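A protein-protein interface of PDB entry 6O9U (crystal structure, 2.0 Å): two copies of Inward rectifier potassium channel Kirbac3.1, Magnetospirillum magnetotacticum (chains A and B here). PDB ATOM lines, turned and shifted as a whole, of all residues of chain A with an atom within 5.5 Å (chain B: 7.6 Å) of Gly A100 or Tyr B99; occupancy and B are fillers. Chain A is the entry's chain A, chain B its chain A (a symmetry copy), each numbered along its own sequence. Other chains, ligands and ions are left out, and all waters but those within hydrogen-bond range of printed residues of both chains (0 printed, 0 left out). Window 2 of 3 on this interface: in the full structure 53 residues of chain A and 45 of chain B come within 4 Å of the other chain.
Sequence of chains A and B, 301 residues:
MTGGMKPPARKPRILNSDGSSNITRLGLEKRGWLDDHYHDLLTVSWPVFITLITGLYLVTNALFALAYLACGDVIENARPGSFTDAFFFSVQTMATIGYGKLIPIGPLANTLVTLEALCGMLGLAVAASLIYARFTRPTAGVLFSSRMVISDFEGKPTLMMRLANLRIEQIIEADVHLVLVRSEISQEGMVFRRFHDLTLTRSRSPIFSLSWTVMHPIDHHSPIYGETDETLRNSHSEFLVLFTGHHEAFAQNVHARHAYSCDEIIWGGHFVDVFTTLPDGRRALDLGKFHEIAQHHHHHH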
ATOM      1  N   ASN A  77      17.931  32.682  22.142  1.00  0.00           N
ATOM      2  CA  ASN A  77      19.065  33.031  22.994  1.00  0.00           C
ATOM      3  C   ASN A  77      20.399  32.560  22.426  1.00  0.00           C
ATOM      4  O   ASN A  77      21.425  32.661  23.111  1.00  0.00           O
ATOM      5  CB  ASN A  77      18.895  32.485  24.416  1.00  0.00           C
ATOM      6  CG  ASN A  77      17.735  33.128  25.147  1.00  0.00           C
ATOM      7  OD1 ASN A  77      17.576  34.348  25.125  1.00  0.00           O
ATOM      8  ND2 ASN A  77      16.914  32.311  25.795  1.00  0.00           N
ATOM      9  N   PHE A  89      23.423  23.569  22.074  1.00  0.00           N
ATOM     10  CA  PHE A  89      21.990  23.297  22.055  1.00  0.00           C
ATOM     11  C   PHE A  89      21.716  21.882  21.564  1.00  0.00           C
ATOM     12  O   PHE A  89      20.822  21.198  22.076  1.00  0.00           O
ATOM     13  CB  PHE A  89      21.264  24.315  21.176  1.00  0.00           C
ATOM     14  CG  PHE A  89      19.835  23.953  20.898  1.00  0.00           C
ATOM     15  CD1 PHE A  89      18.887  24.008  21.904  1.00  0.00           C
ATOM     16  CD2 PHE A  89      19.442  23.547  19.634  1.00  0.00           C
ATOM     17  CE1 PHE A  89      17.574  23.670  21.655  1.00  0.00           C
ATOM     18  CE2 PHE A  89      18.128  23.207  19.380  1.00  0.00           C
ATOM     19  CZ  PHE A  89      17.193  23.268  20.393  1.00  0.00           C
ATOM     20  N   GLN A  92      22.469  19.602  24.485  1.00  0.00           N
ATOM     21  CA  GLN A  92      21.393  19.664  25.466  1.00  0.00           C
ATOM     22  C   GLN A  92      20.126  18.988  24.969  1.00  0.00           C
ATOM     23  O   GLN A  92      19.302  18.565  25.787  1.00  0.00           O
ATOM     24  CB  GLN A  92      21.103  21.123  25.821  1.00  0.00           C
ATOM     25  CG  GLN A  92      22.268  21.835  26.484  1.00  0.00           C
ATOM     26  CD  GLN A  92      22.045  23.329  26.595  1.00  0.00           C
ATOM     27  OE1 GLN A  92      20.919  23.811  26.465  1.00  0.00           O
ATOM     28  NE2 GLN A  92      23.120  24.072  26.832  1.00  0.00           N
ATOM     29  N   THR A  93      19.951  18.876  23.654  1.00  0.00           N
ATOM     30  CA  THR A  93      18.789  18.205  23.085  1.00  0.00           C
ATOM     31  C   THR A  93      19.009  16.699  22.967  1.00  0.00           C
ATOM     32  O   THR A  93      18.157  15.911  23.387  1.00  0.00           O
ATOM     33  CB  THR A  93      18.463  18.811  21.714  1.00  0.00           C
ATOM     34  OG1 THR A  93      18.190  20.212  21.862  1.00  0.00           O
ATOM     35  CG2 THR A  93      17.250  18.135  21.092  1.00  0.00           C
ATOM     36  N   GLY A  98      18.011  19.771  28.285  1.00  0.00           N
ATOM     37  CA  GLY A  98      16.990  20.790  28.135  1.00  0.00           C
ATOM     38  C   GLY A  98      16.989  21.835  29.231  1.00  0.00           C
ATOM     39  O   GLY A  98      15.969  22.028  29.901  1.00  0.00           O
ATOM     40  N   TYR A  99      18.121  22.517  29.428  1.00  0.00           N
ATOM     41  CA  TYR A  99      18.190  23.566  30.443  1.00  0.00           C
ATOM     42  C   TYR A  99      17.039  24.553  30.298  1.00  0.00           C
ATOM     43  O   TYR A  99      16.418  24.947  31.291  1.00  0.00           O
ATOM     44  CB  TYR A  99      19.527  24.306  30.353  1.00  0.00           C
ATOM     45  CG  TYR A  99      20.721  23.529  30.862  1.00  0.00           C
ATOM     46  CD1 TYR A  99      20.773  23.070  32.173  1.00  0.00           C
ATOM     47  CD2 TYR A  99      21.810  23.279  30.039  1.00  0.00           C
ATOM     48  CE1 TYR A  99      21.870  22.369  32.643  1.00  0.00           C
ATOM     49  CE2 TYR A  99      22.913  22.578  30.503  1.00  0.00           C
ATOM     50  CZ  TYR A  99      22.937  22.128  31.804  1.00  0.00           C
ATOM     51  OH  TYR A  99      24.031  21.431  32.265  1.00  0.00           O
ATOM     52  N   GLY A 100      16.737  24.965  29.068  1.00  0.00           N
ATOM     53  CA  GLY A 100      15.629  25.861  28.808  1.00  0.00           C
ATOM     54  C   GLY A 100      16.018  27.255  28.370  1.00  0.00           C
ATOM     55  O   GLY A 100      15.125  28.063  28.090  1.00  0.00           O
ATOM     56  N   LYS A 101      17.313  27.574  28.310  1.00  0.00           N
ATOM     57  CA  LYS A 101      17.734  28.858  27.764  1.00  0.00           C
ATOM     58  C   LYS A 101      17.791  28.804  26.243  1.00  0.00           C
ATOM     59  O   LYS A 101      17.195  29.643  25.559  1.00  0.00           O
ATOM     60  CB  LYS A 101      19.094  29.256  28.341  1.00  0.00           C
ATOM     61  CG  LYS A 101      19.573  30.633  27.905  1.00  0.00           C
ATOM     62  N   LEU A 102      18.497  27.816  25.699  1.00  0.00           N
ATOM     63  CA  LEU A 102      18.497  27.553  24.265  1.00  0.00           C
ATOM     64  C   LEU A 102      17.316  26.641  23.954  1.00  0.00           C
ATOM     65  O   LEU A 102      17.279  25.490  24.403  1.00  0.00           O
ATOM     66  CB  LEU A 102      19.817  26.919  23.834  1.00  0.00           C
ATOM     67  CG  LEU A 102      21.082  27.703  24.188  1.00  0.00           C
ATOM     68  CD1 LEU A 102      22.324  26.856  23.936  1.00  0.00           C
ATOM     69  CD2 LEU A 102      21.151  29.000  23.398  1.00  0.00           C
ATOM     70  N   ILE A 103      16.351  27.154  23.198  1.00  0.00           N
ATOM     71  CA  ILE A 103      15.150  26.394  22.856  1.00  0.00           C
ATOM     72  C   ILE A 103      14.885  26.555  21.366  1.00  0.00           C
ATOM     73  O   ILE A 103      15.299  27.549  20.749  1.00  0.00           O
ATOM     74  CB  ILE A 103      13.931  26.846  23.692  1.00  0.00           C
ATOM     75  CG1 ILE A 103      13.648  28.335  23.473  1.00  0.00           C
ATOM     76  CG2 ILE A 103      14.177  26.558  25.172  1.00  0.00           C
ATOM     77  CD1 ILE A 103      12.354  28.813  24.093  1.00  0.00           C
ATOM     78  N   PRO A 104      14.192  25.595  20.755  1.00  0.00           N
ATOM     79  CA  PRO A 104      13.938  25.670  19.313  1.00  0.00           C
ATOM     80  C   PRO A 104      12.795  26.616  18.976  1.00  0.00           C
ATOM     81  O   PRO A 104      11.857  26.804  19.756  1.00  0.00           O
ATOM     82  CB  PRO A 104      13.582  24.225  18.950  1.00  0.00           C
ATOM     83  CG  PRO A 104      12.929  23.700  20.190  1.00  0.00           C
ATOM     84  CD  PRO A 104      13.643  24.359  21.344  1.00  0.00           C
ATOM     85  N   VAL A 113      14.598  18.634  16.557  1.00  0.00           N
ATOM     86  CA  VAL A 113      14.635  18.216  17.956  1.00  0.00           C
ATOM     87  C   VAL A 113      13.987  16.847  18.116  1.00  0.00           C
ATOM     88  O   VAL A 113      14.511  15.974  18.818  1.00  0.00           O
ATOM     89  CB  VAL A 113      13.955  19.275  18.845  1.00  0.00           C
ATOM     90  CG1 VAL A 113      13.689  18.732  20.248  1.00  0.00           C
ATOM     91  CG2 VAL A 113      14.821  20.521  18.926  1.00  0.00           C
ATOM     92  N   PHE B  88       4.899  18.722  19.926  1.00  0.00           N
ATOM     93  CA  PHE B  88       6.275  18.956  20.342  1.00  0.00           C
ATOM     94  C   PHE B  88       6.404  18.982  21.858  1.00  0.00           C
ATOM     95  O   PHE B  88       7.448  18.590  22.394  1.00  0.00           O
ATOM     96  CB  PHE B  88       6.788  20.253  19.723  1.00  0.00           C
ATOM     97  CG  PHE B  88       6.964  20.180  18.230  1.00  0.00           C
ATOM     98  CD1 PHE B  88       7.647  19.120  17.652  1.00  0.00           C
ATOM     99  CD2 PHE B  88       6.439  21.159  17.404  1.00  0.00           C
ATOM    100  CE1 PHE B  88       7.811  19.046  16.283  1.00  0.00           C
ATOM    101  CE2 PHE B  88       6.600  21.088  16.033  1.00  0.00           C
ATOM    102  CZ  PHE B  88       7.284  20.030  15.472  1.00  0.00           C
ATOM    103  N   VAL B  91       6.694  15.376  22.637  1.00  0.00           N
ATOM    104  CA  VAL B  91       8.068  14.949  22.381  1.00  0.00           C
ATOM    105  C   VAL B  91       8.966  15.340  23.549  1.00  0.00           C
ATOM    106  O   VAL B  91       9.704  14.513  24.095  1.00  0.00           O
ATOM    107  CB  VAL B  91       8.575  15.549  21.057  1.00  0.00           C
ATOM    108  CG1 VAL B  91      10.074  15.328  20.887  1.00  0.00           C
ATOM    109  CG2 VAL B  91       7.815  14.952  19.880  1.00  0.00           C
ATOM    110  N   GLN B  92       8.927  16.616  23.937  1.00  0.00           N
ATOM    111  CA  GLN B  92       9.776  17.099  25.018  1.00  0.00           C
ATOM    112  C   GLN B  92       9.478  16.405  26.335  1.00  0.00           C
ATOM    113  O   GLN B  92      10.349  16.357  27.210  1.00  0.00           O
ATOM    114  CB  GLN B  92       9.604  18.611  25.172  1.00  0.00           C
ATOM    115  CG  GLN B  92      10.041  19.405  23.954  1.00  0.00           C
ATOM    116  CD  GLN B  92       9.630  20.861  24.036  1.00  0.00           C
ATOM    117  OE1 GLN B  92       9.291  21.363  25.107  1.00  0.00           O
ATOM    118  NE2 GLN B  92       9.653  21.546  22.898  1.00  0.00           N
ATOM    119  N   THR B  93       8.272  15.866  26.499  1.00  0.00           N
ATOM    120  CA  THR B  93       7.907  15.142  27.712  1.00  0.00           C
ATOM    121  C   THR B  93       8.315  13.672  27.635  1.00  0.00           C
ATOM    122  O   THR B  93       8.937  13.151  28.565  1.00  0.00           O
ATOM    123  CB  THR B  93       6.399  15.270  27.955  1.00  0.00           C
ATOM    124  OG1 THR B  93       6.050  16.655  28.096  1.00  0.00           O
ATOM    125  CG2 THR B  93       5.985  14.528  29.217  1.00  0.00           C
ATOM    126  N   THR B  96      11.819  13.397  27.700  1.00  0.00           N
ATOM    127  CA  THR B  96      12.290  13.970  28.961  1.00  0.00           C
ATOM    128  C   THR B  96      13.267  15.122  28.742  1.00  0.00           C
ATOM    129  O   THR B  96      14.140  15.376  29.572  1.00  0.00           O
ATOM    130  CB  THR B  96      12.921  12.897  29.862  1.00  0.00           C
ATOM    131  OG1 THR B  96      14.054  12.314  29.209  1.00  0.00           O
ATOM    132  CG2 THR B  96      11.909  11.807  30.186  1.00  0.00           C
ATOM    133  N   ILE B  97      13.123  15.848  27.630  1.00  0.00           N
ATOM    134  CA  ILE B  97      13.944  17.037  27.415  1.00  0.00           C
ATOM    135  C   ILE B  97      13.523  18.146  28.374  1.00  0.00           C
ATOM    136  O   ILE B  97      14.359  18.740  29.064  1.00  0.00           O
ATOM    137  CB  ILE B  97      13.851  17.500  25.951  1.00  0.00           C
ATOM    138  CG1 ILE B  97      14.281  16.380  25.003  1.00  0.00           C
ATOM    139  CG2 ILE B  97      14.722  18.733  25.726  1.00  0.00           C
ATOM    140  CD1 ILE B  97      13.985  16.665  23.549  1.00  0.00           C
ATOM    141  N   GLY B  98      12.227  18.448  28.419  1.00  0.00           N
ATOM    142  CA  GLY B  98      11.694  19.437  29.335  1.00  0.00           C
ATOM    143  C   GLY B  98      12.371  20.789  29.253  1.00  0.00           C
ATOM    144  O   GLY B  98      12.887  21.285  30.260  1.00  0.00           O
ATOM    145  N   TYR B  99      12.380  21.399  28.064  1.00  0.00           N
ATOM    146  CA  TYR B  99      12.981  22.721  27.911  1.00  0.00           C
ATOM    147  C   TYR B  99      12.457  23.694  28.960  1.00  0.00           C
ATOM    148  O   TYR B  99      13.227  24.454  29.557  1.00  0.00           O
ATOM    149  CB  TYR B  99      12.711  23.270  26.508  1.00  0.00           C
ATOM    150  CG  TYR B  99      13.510  22.615  25.403  1.00  0.00           C
ATOM    151  CD1 TYR B  99      14.899  22.628  25.417  1.00  0.00           C
ATOM    152  CD2 TYR B  99      12.873  22.008  24.330  1.00  0.00           C
ATOM    153  CE1 TYR B  99      15.630  22.039  24.398  1.00  0.00           C
ATOM    154  CE2 TYR B  99      13.598  21.417  23.307  1.00  0.00           C
ATOM    155  CZ  TYR B  99      14.974  21.437  23.346  1.00  0.00           C
ATOM    156  OH  TYR B  99      15.694  20.849  22.332  1.00  0.00           O
ATOM    157  N   GLY B 100      11.148  23.685  29.202  1.00  0.00           N
ATOM    158  CA  GLY B 100      10.547  24.529  30.215  1.00  0.00           C
ATOM    159  C   GLY B 100       9.683  25.652  29.687  1.00  0.00           C
ATOM    160  O   GLY B 100       9.103  26.389  30.493  1.00  0.00           O
ATOM    161  N   LYS B 101       9.581  25.820  28.366  1.00  0.00           N
ATOM    162  CA  LYS B 101       8.653  26.801  27.815  1.00  0.00           C
ATOM    163  C   LYS B 101       7.244  26.226  27.739  1.00  0.00           C
ATOM    164  O   LYS B 101       6.289  26.829  28.241  1.00  0.00           O
ATOM    165  CB  LYS B 101       9.125  27.255  26.433  1.00  0.00           C
ATOM    166  CG  LYS B 101       8.273  28.355  25.816  1.00  0.00           C
ATOM    167  N   LEU B 102       7.101  25.056  27.123  1.00  0.00           N
ATOM    168  CA  LEU B 102       5.841  24.321  27.124  1.00  0.00           C
ATOM    169  C   LEU B 102       5.802  23.461  28.382  1.00  0.00           C
ATOM    170  O   LEU B 102       6.610  22.539  28.536  1.00  0.00           O
ATOM    171  CB  LEU B 102       5.714  23.468  25.863  1.00  0.00           C
ATOM    172  CG  LEU B 102       5.842  24.215  24.536  1.00  0.00           C
ATOM    173  CD1 LEU B 102       5.951  23.232  23.377  1.00  0.00           C
ATOM    174  CD2 LEU B 102       4.665  25.155  24.330  1.00  0.00           C
ATOM    175  N   ILE B 103       4.872  23.766  29.280  1.00  0.00           N
ATOM    176  CA  ILE B 103       4.750  23.039  30.544  1.00  0.00           C
ATOM    177  C   ILE B 103       3.282  22.704  30.769  1.00  0.00           C
ATOM    178  O   ILE B 103       2.385  23.388  30.252  1.00  0.00           O
ATOM    179  CB  ILE B 103       5.325  23.851  31.727  1.00  0.00           C
ATOM    180  CG1 ILE B 103       4.601  25.194  31.861  1.00  0.00           C
ATOM    181  CG2 ILE B 103       6.825  24.065  31.533  1.00  0.00           C
ATOM    182  CD1 ILE B 103       4.961  25.963  33.115  1.00  0.00           C
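OG1 of Thr A93 is in hydrogen-bond range of OH of Tyr B99 (2.6 Å). The backbone carbonyl oxygen (O) of Gly A98 lies close to the backbone carbonyl oxygen (O) of Gly B98, at 3.2 Å.
O of Gln B92 lies within hydrogen-bond range of N of Ile B97 (2.9 Å). The backbone carbonyl oxygen (O) of Gln A92 is in hydrogen-bond range of the backbone NH (N) of Gly A98, at 3.1 Å. The backbone carbonyl oxygen of Gln B92 is in hydrogen-bond range of the backbone NH of Gly B98 (3.1 Å). O of Phe A89 lies within hydrogen-bond range of OG1 of Thr A93 (2.8 Å).
CZ of Phe A89 touches OH of Tyr B99 (3.4 Å). O of Ile B97 touches CA of Gly A98 (3.5 Å). Gly A98 touches Tyr B99 (O to CA, 3.7 Å). Tyr A99 touches Tyr B99 (O to O, 3.7 Å). Gly A100 touches Tyr B99 (CA to O, 2.9 Å). Leu A102 touches Tyr B99. Ile A103 touches Tyr B99. CE2 of Tyr B99 touches CD of Pro A104, at 3.5 Å. CD1 of Ile B97 touches CG1 of Val A113, 3.9 Å away. Tyr B99 touches Val A113.
Gly A100 touches just one residue of chain B: Tyr B99 (2.9 Å). Of chain A, only Phe A89 (3.4 Å), Thr A93 (2.6 Å), Gly A98 (3.7 Å), Tyr A99 (3.7 Å), Gly A100 (2.9 Å), Leu A102 (3.8 Å), Ile A103 (3.8 Å), Pro A104 (3.5 Å) and Val A113 (3.5 Å) come within 4 Å of Tyr B99. Of the printed residues of chain B, Phe A89 touches Tyr B99. Printed residues of chain B within 4 Å of Thr A93: Tyr B99 (2.6 Å). Printed residues of chain B within 4 Å of Pro A104: Tyr B99 (3.5 Å). Printed residues of chain A within 4 Å of Gly B98: Gly A98. The nearest residue of chain B that does not touch Gly A100 is Gly B100 (5.0 Å). The nearest printed residue of chain A that does not touch Ile B97 is Thr A93 (4.2 Å).
Of the 12 printed residues of chain B, 3 touch a printed residue of chain A. Printed residues of chain B that touch a printed residue of chain A: Ile B97, Gly B98 and Tyr B99. Along chain B the printed residues that touch a printed residue of chain A span positions 97 to 99.
Thr A93 touches Tyr B99, but with the chains exchanged Tyr A99 does not touch Thr B93 (12.2 Å). Gly A98 touches its own counterpart, Gly B98. Tyr B99 touches its own counterpart, Tyr A99. Leu A102 touches Tyr B99, but with the chains exchanged Tyr A99 does not touch Leu B102 (10.2 Å). Positions printed for both chains: 92, 93, 98, 99, 100, 101, 102 and 103.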
